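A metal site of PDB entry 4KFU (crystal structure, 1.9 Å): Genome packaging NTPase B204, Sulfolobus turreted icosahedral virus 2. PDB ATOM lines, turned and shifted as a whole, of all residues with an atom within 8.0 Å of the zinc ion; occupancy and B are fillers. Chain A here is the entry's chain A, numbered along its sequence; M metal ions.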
ATOM      1  N   ILE A  38      20.404 -16.808  18.631  1.00  0.00           N
ATOM      2  CA  ILE A  38      20.738 -17.048  20.039  1.00  0.00           C
ATOM      3  C   ILE A  38      21.952 -17.960  20.217  1.00  0.00           C
ATOM      4  O   ILE A  38      21.944 -19.127  19.795  1.00  0.00           O
ATOM      5  CB  ILE A  38      19.553 -17.672  20.807  1.00  0.00           C
ATOM      6  CG1 ILE A  38      18.278 -16.831  20.627  1.00  0.00           C
ATOM      7  CG2 ILE A  38      19.901 -17.835  22.280  1.00  0.00           C
ATOM      8  CD1 ILE A  38      17.028 -17.462  21.262  1.00  0.00           C
ATOM      9  N   ASP A  39      22.985 -17.418  20.855  1.00  0.00           N
ATOM     10  CA  ASP A  39      24.186 -18.165  21.243  1.00  0.00           C
ATOM     11  C   ASP A  39      23.920 -18.783  22.608  1.00  0.00           C
ATOM     12  O   ASP A  39      23.967 -18.090  23.634  1.00  0.00           O
ATOM     13  CB  ASP A  39      25.399 -17.210  21.255  1.00  0.00           C
ATOM     14  CG  ASP A  39      26.688 -17.871  21.749  1.00  0.00           C
ATOM     15  OD1 ASP A  39      26.802 -19.112  21.742  1.00  0.00           O
ATOM     16  OD2 ASP A  39      27.618 -17.124  22.148  1.00  0.00           O
ATOM     17  N   ASP A  40      23.624 -20.078  22.621  1.00  0.00           N
ATOM     18  CA  ASP A  40      23.110 -20.805  23.802  1.00  0.00           C
ATOM     19  C   ASP A  40      24.197 -21.721  24.380  1.00  0.00           C
ATOM     20  O   ASP A  40      24.780 -22.548  23.655  1.00  0.00           O
ATOM     21  CB  ASP A  40      21.894 -21.629  23.376  1.00  0.00           C
ATOM     22  CG  ASP A  40      21.063 -22.164  24.563  1.00  0.00           C
ATOM     23  OD1 ASP A  40      21.565 -22.232  25.708  1.00  0.00           O
ATOM     24  OD2 ASP A  40      19.897 -22.525  24.326  1.00  0.00           O
ATOM     25  N   HIS A  41      24.456 -21.618  25.679  1.00  0.00           N
ATOM     26  CA  HIS A  41      25.519 -22.406  26.303  1.00  0.00           C
ATOM     27  C   HIS A  41      24.999 -23.471  27.269  1.00  0.00           C
ATOM     28  O   HIS A  41      25.782 -24.260  27.800  1.00  0.00           O
ATOM     29  CB  HIS A  41      26.505 -21.475  27.011  1.00  0.00           C
ATOM     30  CG  HIS A  41      27.048 -20.404  26.113  1.00  0.00           C
ATOM     31  ND1 HIS A  41      26.517 -19.135  26.074  1.00  0.00           N
ATOM     32  CD2 HIS A  41      28.042 -20.429  25.195  1.00  0.00           C
ATOM     33  CE1 HIS A  41      27.175 -18.407  25.187  1.00  0.00           C
ATOM     34  NE2 HIS A  41      28.106 -19.171  24.635  1.00  0.00           N
ATOM     35  N   VAL A  71      21.775 -21.438  18.299  1.00  0.00           N
ATOM     36  CA  VAL A  71      23.048 -22.102  18.123  1.00  0.00           C
ATOM     37  C   VAL A  71      23.528 -22.605  19.480  1.00  0.00           C
ATOM     38  O   VAL A  71      23.856 -21.793  20.351  1.00  0.00           O
ATOM     39  CB  VAL A  71      24.119 -21.117  17.602  1.00  0.00           C
ATOM     40  CG1 VAL A  71      25.341 -21.873  17.098  1.00  0.00           C
ATOM     41  CG2 VAL A  71      23.531 -20.216  16.509  1.00  0.00           C
ATOM     42  N   TYR A  72      23.601 -23.913  19.672  1.00  0.00           N
ATOM     43  CA  TYR A  72      24.224 -24.412  20.889  1.00  0.00           C
ATOM     44  C   TYR A  72      25.744 -24.318  20.770  1.00  0.00           C
ATOM     45  O   TYR A  72      26.336 -24.883  19.840  1.00  0.00           O
ATOM     46  CB  TYR A  72      23.828 -25.848  21.217  1.00  0.00           C
ATOM     47  CG  TYR A  72      24.646 -26.391  22.368  1.00  0.00           C
ATOM     48  CD1 TYR A  72      24.449 -25.922  23.652  1.00  0.00           C
ATOM     49  CD2 TYR A  72      25.644 -27.332  22.148  1.00  0.00           C
ATOM     50  CE1 TYR A  72      25.217 -26.382  24.717  1.00  0.00           C
ATOM     51  CE2 TYR A  72      26.420 -27.814  23.202  1.00  0.00           C
ATOM     52  CZ  TYR A  72      26.198 -27.333  24.482  1.00  0.00           C
ATOM     53  OH  TYR A  72      26.960 -27.795  25.534  1.00  0.00           O
ATOM     54  N   ASP A  73      26.385 -23.624  21.707  1.00  0.00           N
ATOM     55  CA  ASP A  73      27.834 -23.406  21.672  1.00  0.00           C
ATOM     56  C   ASP A  73      28.578 -24.331  22.621  1.00  0.00           C
ATOM     57  O   ASP A  73      28.605 -24.095  23.838  1.00  0.00           O
ATOM     58  CB  ASP A  73      28.154 -21.936  21.992  1.00  0.00           C
ATOM     59  CG  ASP A  73      29.646 -21.652  22.056  1.00  0.00           C
ATOM     60  OD1 ASP A  73      30.471 -22.468  21.576  1.00  0.00           O
ATOM     61  OD2 ASP A  73      30.009 -20.587  22.592  1.00  0.00           O
ATOM     62  N   ARG A  74      29.191 -25.368  22.053  1.00  0.00           N
ATOM     63  CA  ARG A  74      29.857 -26.403  22.823  1.00  0.00           C
ATOM     64  C   ARG A  74      31.270 -25.990  23.251  1.00  0.00           C
ATOM     65  O   ARG A  74      31.651 -26.172  24.402  1.00  0.00           O
ATOM     66  CB  ARG A  74      29.911 -27.702  21.999  1.00  0.00           C
ATOM     67  CG  ARG A  74      30.796 -28.791  22.589  1.00  0.00           C
ATOM     68  N   ALA A  75      32.022 -25.424  22.319  1.00  0.00           N
ATOM     69  CA  ALA A  75      33.419 -25.029  22.575  1.00  0.00           C
ATOM     70  C   ALA A  75      33.561 -23.836  23.528  1.00  0.00           C
ATOM     71  O   ALA A  75      34.549 -23.772  24.276  1.00  0.00           O
ATOM     72  CB  ALA A  75      34.131 -24.748  21.258  1.00  0.00           C
ATOM     73  N   LYS A  76      32.610 -22.916  23.476  1.00  0.00           N
ATOM     74  CA  LYS A  76      32.581 -21.718  24.353  1.00  0.00           C
ATOM     75  C   LYS A  76      33.872 -20.919  24.336  1.00  0.00           C
ATOM     76  O   LYS A  76      34.299 -20.388  25.377  1.00  0.00           O
ATOM     77  CB  LYS A  76      32.230 -22.122  25.793  1.00  0.00           C
ATOM     78  CG  LYS A  76      30.881 -22.830  25.915  1.00  0.00           C
ATOM     79  CD  LYS A  76      30.793 -23.652  27.192  1.00  0.00           C
ATOM     80  CE  LYS A  76      29.434 -24.325  27.324  1.00  0.00           C
ATOM     81  NZ  LYS A  76      29.125 -25.184  26.141  1.00  0.00           N
ATOM     82  N   ASN A  77      34.488 -20.808  23.153  1.00  0.00           N
ATOM     83  CA  ASN A  77      35.795 -20.162  23.025  1.00  0.00           C
ATOM     84  C   ASN A  77      35.840 -18.975  22.048  1.00  0.00           C
ATOM     85  O   ASN A  77      34.844 -18.666  21.377  1.00  0.00           O
ATOM     86  CB  ASN A  77      36.875 -21.193  22.657  1.00  0.00           C
ATOM     87  CG  ASN A  77      36.572 -21.943  21.350  1.00  0.00           C
ATOM     88  OD1 ASN A  77      35.707 -21.546  20.552  1.00  0.00           O
ATOM     89  ND2 ASN A  77      37.292 -23.045  21.123  1.00  0.00           N
ATOM     90  N   PHE A  80      35.025 -19.711  18.291  1.00  0.00           N
ATOM     91  CA  PHE A  80      33.622 -19.902  17.993  1.00  0.00           C
ATOM     92  C   PHE A  80      32.927 -18.558  17.837  1.00  0.00           C
ATOM     93  O   PHE A  80      32.184 -18.375  16.884  1.00  0.00           O
ATOM     94  CB  PHE A  80      32.912 -20.736  19.050  1.00  0.00           C
ATOM     95  CG  PHE A  80      31.468 -21.020  18.718  1.00  0.00           C
ATOM     96  CD1 PHE A  80      31.136 -22.127  17.942  1.00  0.00           C
ATOM     97  CD2 PHE A  80      30.456 -20.171  19.143  1.00  0.00           C
ATOM     98  CE1 PHE A  80      29.817 -22.388  17.619  1.00  0.00           C
ATOM     99  CE2 PHE A  80      29.133 -20.426  18.813  1.00  0.00           C
ATOM    100  CZ  PHE A  80      28.820 -21.537  18.052  1.00  0.00           C
ATOM    101  N   PHE A  81      33.147 -17.642  18.781  1.00  0.00           N
ATOM    102  CA  PHE A  81      32.460 -16.344  18.680  1.00  0.00           C
ATOM    103  C   PHE A  81      32.838 -15.639  17.378  1.00  0.00           C
ATOM    104  O   PHE A  81      31.991 -15.012  16.730  1.00  0.00           O
ATOM    105  CB  PHE A  81      32.714 -15.427  19.875  1.00  0.00           C
ATOM    106  CG  PHE A  81      32.001 -14.112  19.747  1.00  0.00           C
ATOM    107  CD1 PHE A  81      30.625 -14.028  19.967  1.00  0.00           C
ATOM    108  CD2 PHE A  81      32.667 -12.978  19.318  1.00  0.00           C
ATOM    109  CE1 PHE A  81      29.949 -12.825  19.801  1.00  0.00           C
ATOM    110  CE2 PHE A  81      31.997 -11.781  19.141  1.00  0.00           C
ATOM    111  CZ  PHE A  81      30.632 -11.702  19.381  1.00  0.00           C
ATOM    112  N   LEU A  84      30.844 -17.172  14.640  1.00  0.00           N
ATOM    113  CA  LEU A  84      29.440 -16.794  14.813  1.00  0.00           C
ATOM    114  C   LEU A  84      29.166 -15.355  14.397  1.00  0.00           C
ATOM    115  O   LEU A  84      28.111 -15.040  13.857  1.00  0.00           O
ATOM    116  CB  LEU A  84      29.026 -16.990  16.278  1.00  0.00           C
ATOM    117  CG  LEU A  84      27.653 -16.454  16.704  1.00  0.00           C
ATOM    118  CD1 LEU A  84      26.543 -17.139  15.928  1.00  0.00           C
ATOM    119  CD2 LEU A  84      27.418 -16.621  18.197  1.00  0.00           C
ATOM    120  N   ILE A 101      21.665 -12.587  20.464  1.00  0.00           N
ATOM    121  CA  ILE A 101      21.422 -12.823  21.882  1.00  0.00           C
ATOM    122  C   ILE A 101      22.389 -13.830  22.472  1.00  0.00           C
ATOM    123  O   ILE A 101      22.484 -14.973  22.014  1.00  0.00           O
ATOM    124  CB  ILE A 101      19.992 -13.342  22.127  1.00  0.00           C
ATOM    125  CG1 ILE A 101      18.969 -12.439  21.425  1.00  0.00           C
ATOM    126  CG2 ILE A 101      19.703 -13.450  23.633  1.00  0.00           C
ATOM    127  CD1 ILE A 101      17.506 -12.796  21.724  1.00  0.00           C
ATOM    128  N   ILE A 102      23.119 -13.399  23.495  1.00  0.00           N
ATOM    129  CA  ILE A 102      24.169 -14.212  24.089  1.00  0.00           C
ATOM    130  C   ILE A 102      23.910 -14.403  25.573  1.00  0.00           C
ATOM    131  O   ILE A 102      24.228 -13.531  26.387  1.00  0.00           O
ATOM    132  CB  ILE A 102      25.551 -13.581  23.903  1.00  0.00           C
ATOM    133  CG1 ILE A 102      25.734 -13.155  22.447  1.00  0.00           C
ATOM    134  CG2 ILE A 102      26.674 -14.580  24.291  1.00  0.00           C
ATOM    135  CD1 ILE A 102      27.150 -12.842  22.088  1.00  0.00           C
ATOM    136  N   ASP A 103      23.297 -15.535  25.928  1.00  0.00           N
ATOM    137  CA  ASP A 103      23.115 -15.849  27.340  1.00  0.00           C
ATOM    138  C   ASP A 103      24.433 -16.412  27.865  1.00  0.00           C
ATOM    139  O   ASP A 103      25.246 -16.930  27.077  1.00  0.00           O
ATOM    140  CB  ASP A 103      21.952 -16.808  27.564  1.00  0.00           C
ATOM    141  CG  ASP A 103      21.088 -16.399  28.774  1.00  0.00           C
ATOM    142  OD1 ASP A 103      21.645 -15.798  29.729  1.00  0.00           O
ATOM    143  OD2 ASP A 103      19.860 -16.678  28.771  1.00  0.00           O
ATOM    144  N   GLU A 104      24.679 -16.267  29.167  1.00  0.00           N
ATOM    145  CA  GLU A 104      25.971 -16.632  29.748  1.00  0.00           C
ATOM    146  C   GLU A 104      27.129 -15.961  28.980  1.00  0.00           C
ATOM    147  O   GLU A 104      28.091 -16.629  28.577  1.00  0.00           O
ATOM    148  CB  GLU A 104      26.146 -18.157  29.763  1.00  0.00           C
ATOM    149  CG  GLU A 104      24.965 -18.936  30.395  1.00  0.00           C
ATOM    150  CD  GLU A 104      23.876 -19.358  29.394  1.00  0.00           C
ATOM    151  OE1 GLU A 104      24.168 -19.472  28.170  1.00  0.00           O
ATOM    152  OE2 GLU A 104      22.723 -19.595  29.824  1.00  0.00           O
ATOM    153  N   ALA A 105      27.029 -14.649  28.777  1.00  0.00           N
ATOM    154  CA  ALA A 105      27.990 -13.941  27.935  1.00  0.00           C
ATOM    155  C   ALA A 105      29.416 -13.893  28.457  1.00  0.00           C
ATOM    156  O   ALA A 105      30.309 -13.436  27.744  1.00  0.00           O
ATOM    157  CB  ALA A 105      27.496 -12.523  27.611  1.00  0.00           C
ATOM    158  N   TYR A 107      31.365 -16.221  28.652  1.00  0.00           N
ATOM    159  CA  TYR A 107      32.218 -17.106  27.851  1.00  0.00           C
ATOM    160  C   TYR A 107      33.014 -16.354  26.816  1.00  0.00           C
ATOM    161  O   TYR A 107      34.134 -16.729  26.496  1.00  0.00           O
ATOM    162  CB  TYR A 107      31.391 -18.195  27.185  1.00  0.00           C
ATOM    163  CG  TYR A 107      30.908 -19.219  28.168  1.00  0.00           C
ATOM    164  CD1 TYR A 107      31.824 -20.006  28.879  1.00  0.00           C
ATOM    165  CD2 TYR A 107      29.562 -19.379  28.423  1.00  0.00           C
ATOM    166  CE1 TYR A 107      31.382 -20.942  29.801  1.00  0.00           C
ATOM    167  CE2 TYR A 107      29.116 -20.309  29.339  1.00  0.00           C
ATOM    168  CZ  TYR A 107      30.021 -21.091  30.031  1.00  0.00           C
ATOM    169  OH  TYR A 107      29.565 -22.008  30.950  1.00  0.00           O
ATOM    170  N   HIS A 108      32.437 -15.270  26.282  1.00  0.00           N
ATOM    171  CA  HIS A 108      33.056 -14.550  25.155  1.00  0.00           C
ATOM    172  C   HIS A 108      33.514 -13.140  25.516  1.00  0.00           C
ATOM    173  O   HIS A 108      34.307 -12.539  24.789  1.00  0.00           O
ATOM    174  CB  HIS A 108      32.065 -14.483  23.993  1.00  0.00           C
ATOM    175  CG  HIS A 108      31.594 -15.820  23.528  1.00  0.00           C
ATOM    176  ND1 HIS A 108      32.463 -16.870  23.295  1.00  0.00           N
ATOM    177  CD2 HIS A 108      30.360 -16.284  23.248  1.00  0.00           C
ATOM    178  CE1 HIS A 108      31.775 -17.923  22.898  1.00  0.00           C
ATOM    179  NE2 HIS A 108      30.504 -17.596  22.855  1.00  0.00           N
ATOM    180  N   PHE A 109      32.986 -12.611  26.615  1.00  0.00           N
ATOM    181  CA  PHE A 109      33.271 -11.227  27.007  1.00  0.00           C
ATOM    182  C   PHE A 109      33.808 -11.150  28.435  1.00  0.00           C
ATOM    183  O   PHE A 109      33.553 -10.191  29.170  1.00  0.00           O
ATOM    184  CB  PHE A 109      32.003 -10.389  26.910  1.00  0.00           C
ATOM    185  CG  PHE A 109      31.465 -10.223  25.505  1.00  0.00           C
ATOM    186  CD1 PHE A 109      30.699 -11.230  24.913  1.00  0.00           C
ATOM    187  CD2 PHE A 109      31.676  -9.048  24.796  1.00  0.00           C
ATOM    188  CE1 PHE A 109      30.173 -11.071  23.645  1.00  0.00           C
ATOM    189  CE2 PHE A 109      31.168  -8.887  23.519  1.00  0.00           C
ATOM    190  CZ  PHE A 109      30.421  -9.898  22.941  1.00  0.00           C
HETATM  191 ZN    ZN M   1      28.932 -18.875  22.756  1.00  0.00          ZN
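The nearest printed residue that does not touch the zinc ion is Phe 80 (4.1 Å).
NE2 of His 108 is bound to the zinc ion, at 2.0 Å.
The zinc ion is bound by the side-chain carboxylate (OD2) of Asp 73.
NE2 of His 41 is bound to the zinc ion (2.1 Å).
The zinc ion is bound by the side-chain carboxylate (OD2) of Asp 39 (2.3 Å).
The zinc ion is bound by OD1 of Asp 39 (2.4 Å).
The zinc ion has five donor atoms within binding distance.
N of Ala 75 is in hydrogen-bond range of OD1 of Asp 73.
The backbone carbonyl oxygen (O) of Asp 73 sits at hydrogen-bond distance from the side-chain amino group (NZ) of Lys 76 (2.6 Å).
O of Asp 39 is in hydrogen-bond range of N of Asp 103 (3.5 Å).
A ring nitrogen (ND1) of His 41 sits at hydrogen-bond distance from the backbone carbonyl oxygen of Asp 103 (2.7 Å).
A ring nitrogen (ND1) of His 41 is in hydrogen-bond range of the side-chain carboxylate (OE1) of Glu 104, 3.2 Å away.
The backbone NH of Asp 73 is in hydrogen-bond range of the backbone carbonyl oxygen of Asp 40 (2.7 Å).
The backbone NH (N) of Asp 39 is in hydrogen-bond range of the backbone carbonyl oxygen (O) of Ile 101 (2.8 Å).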
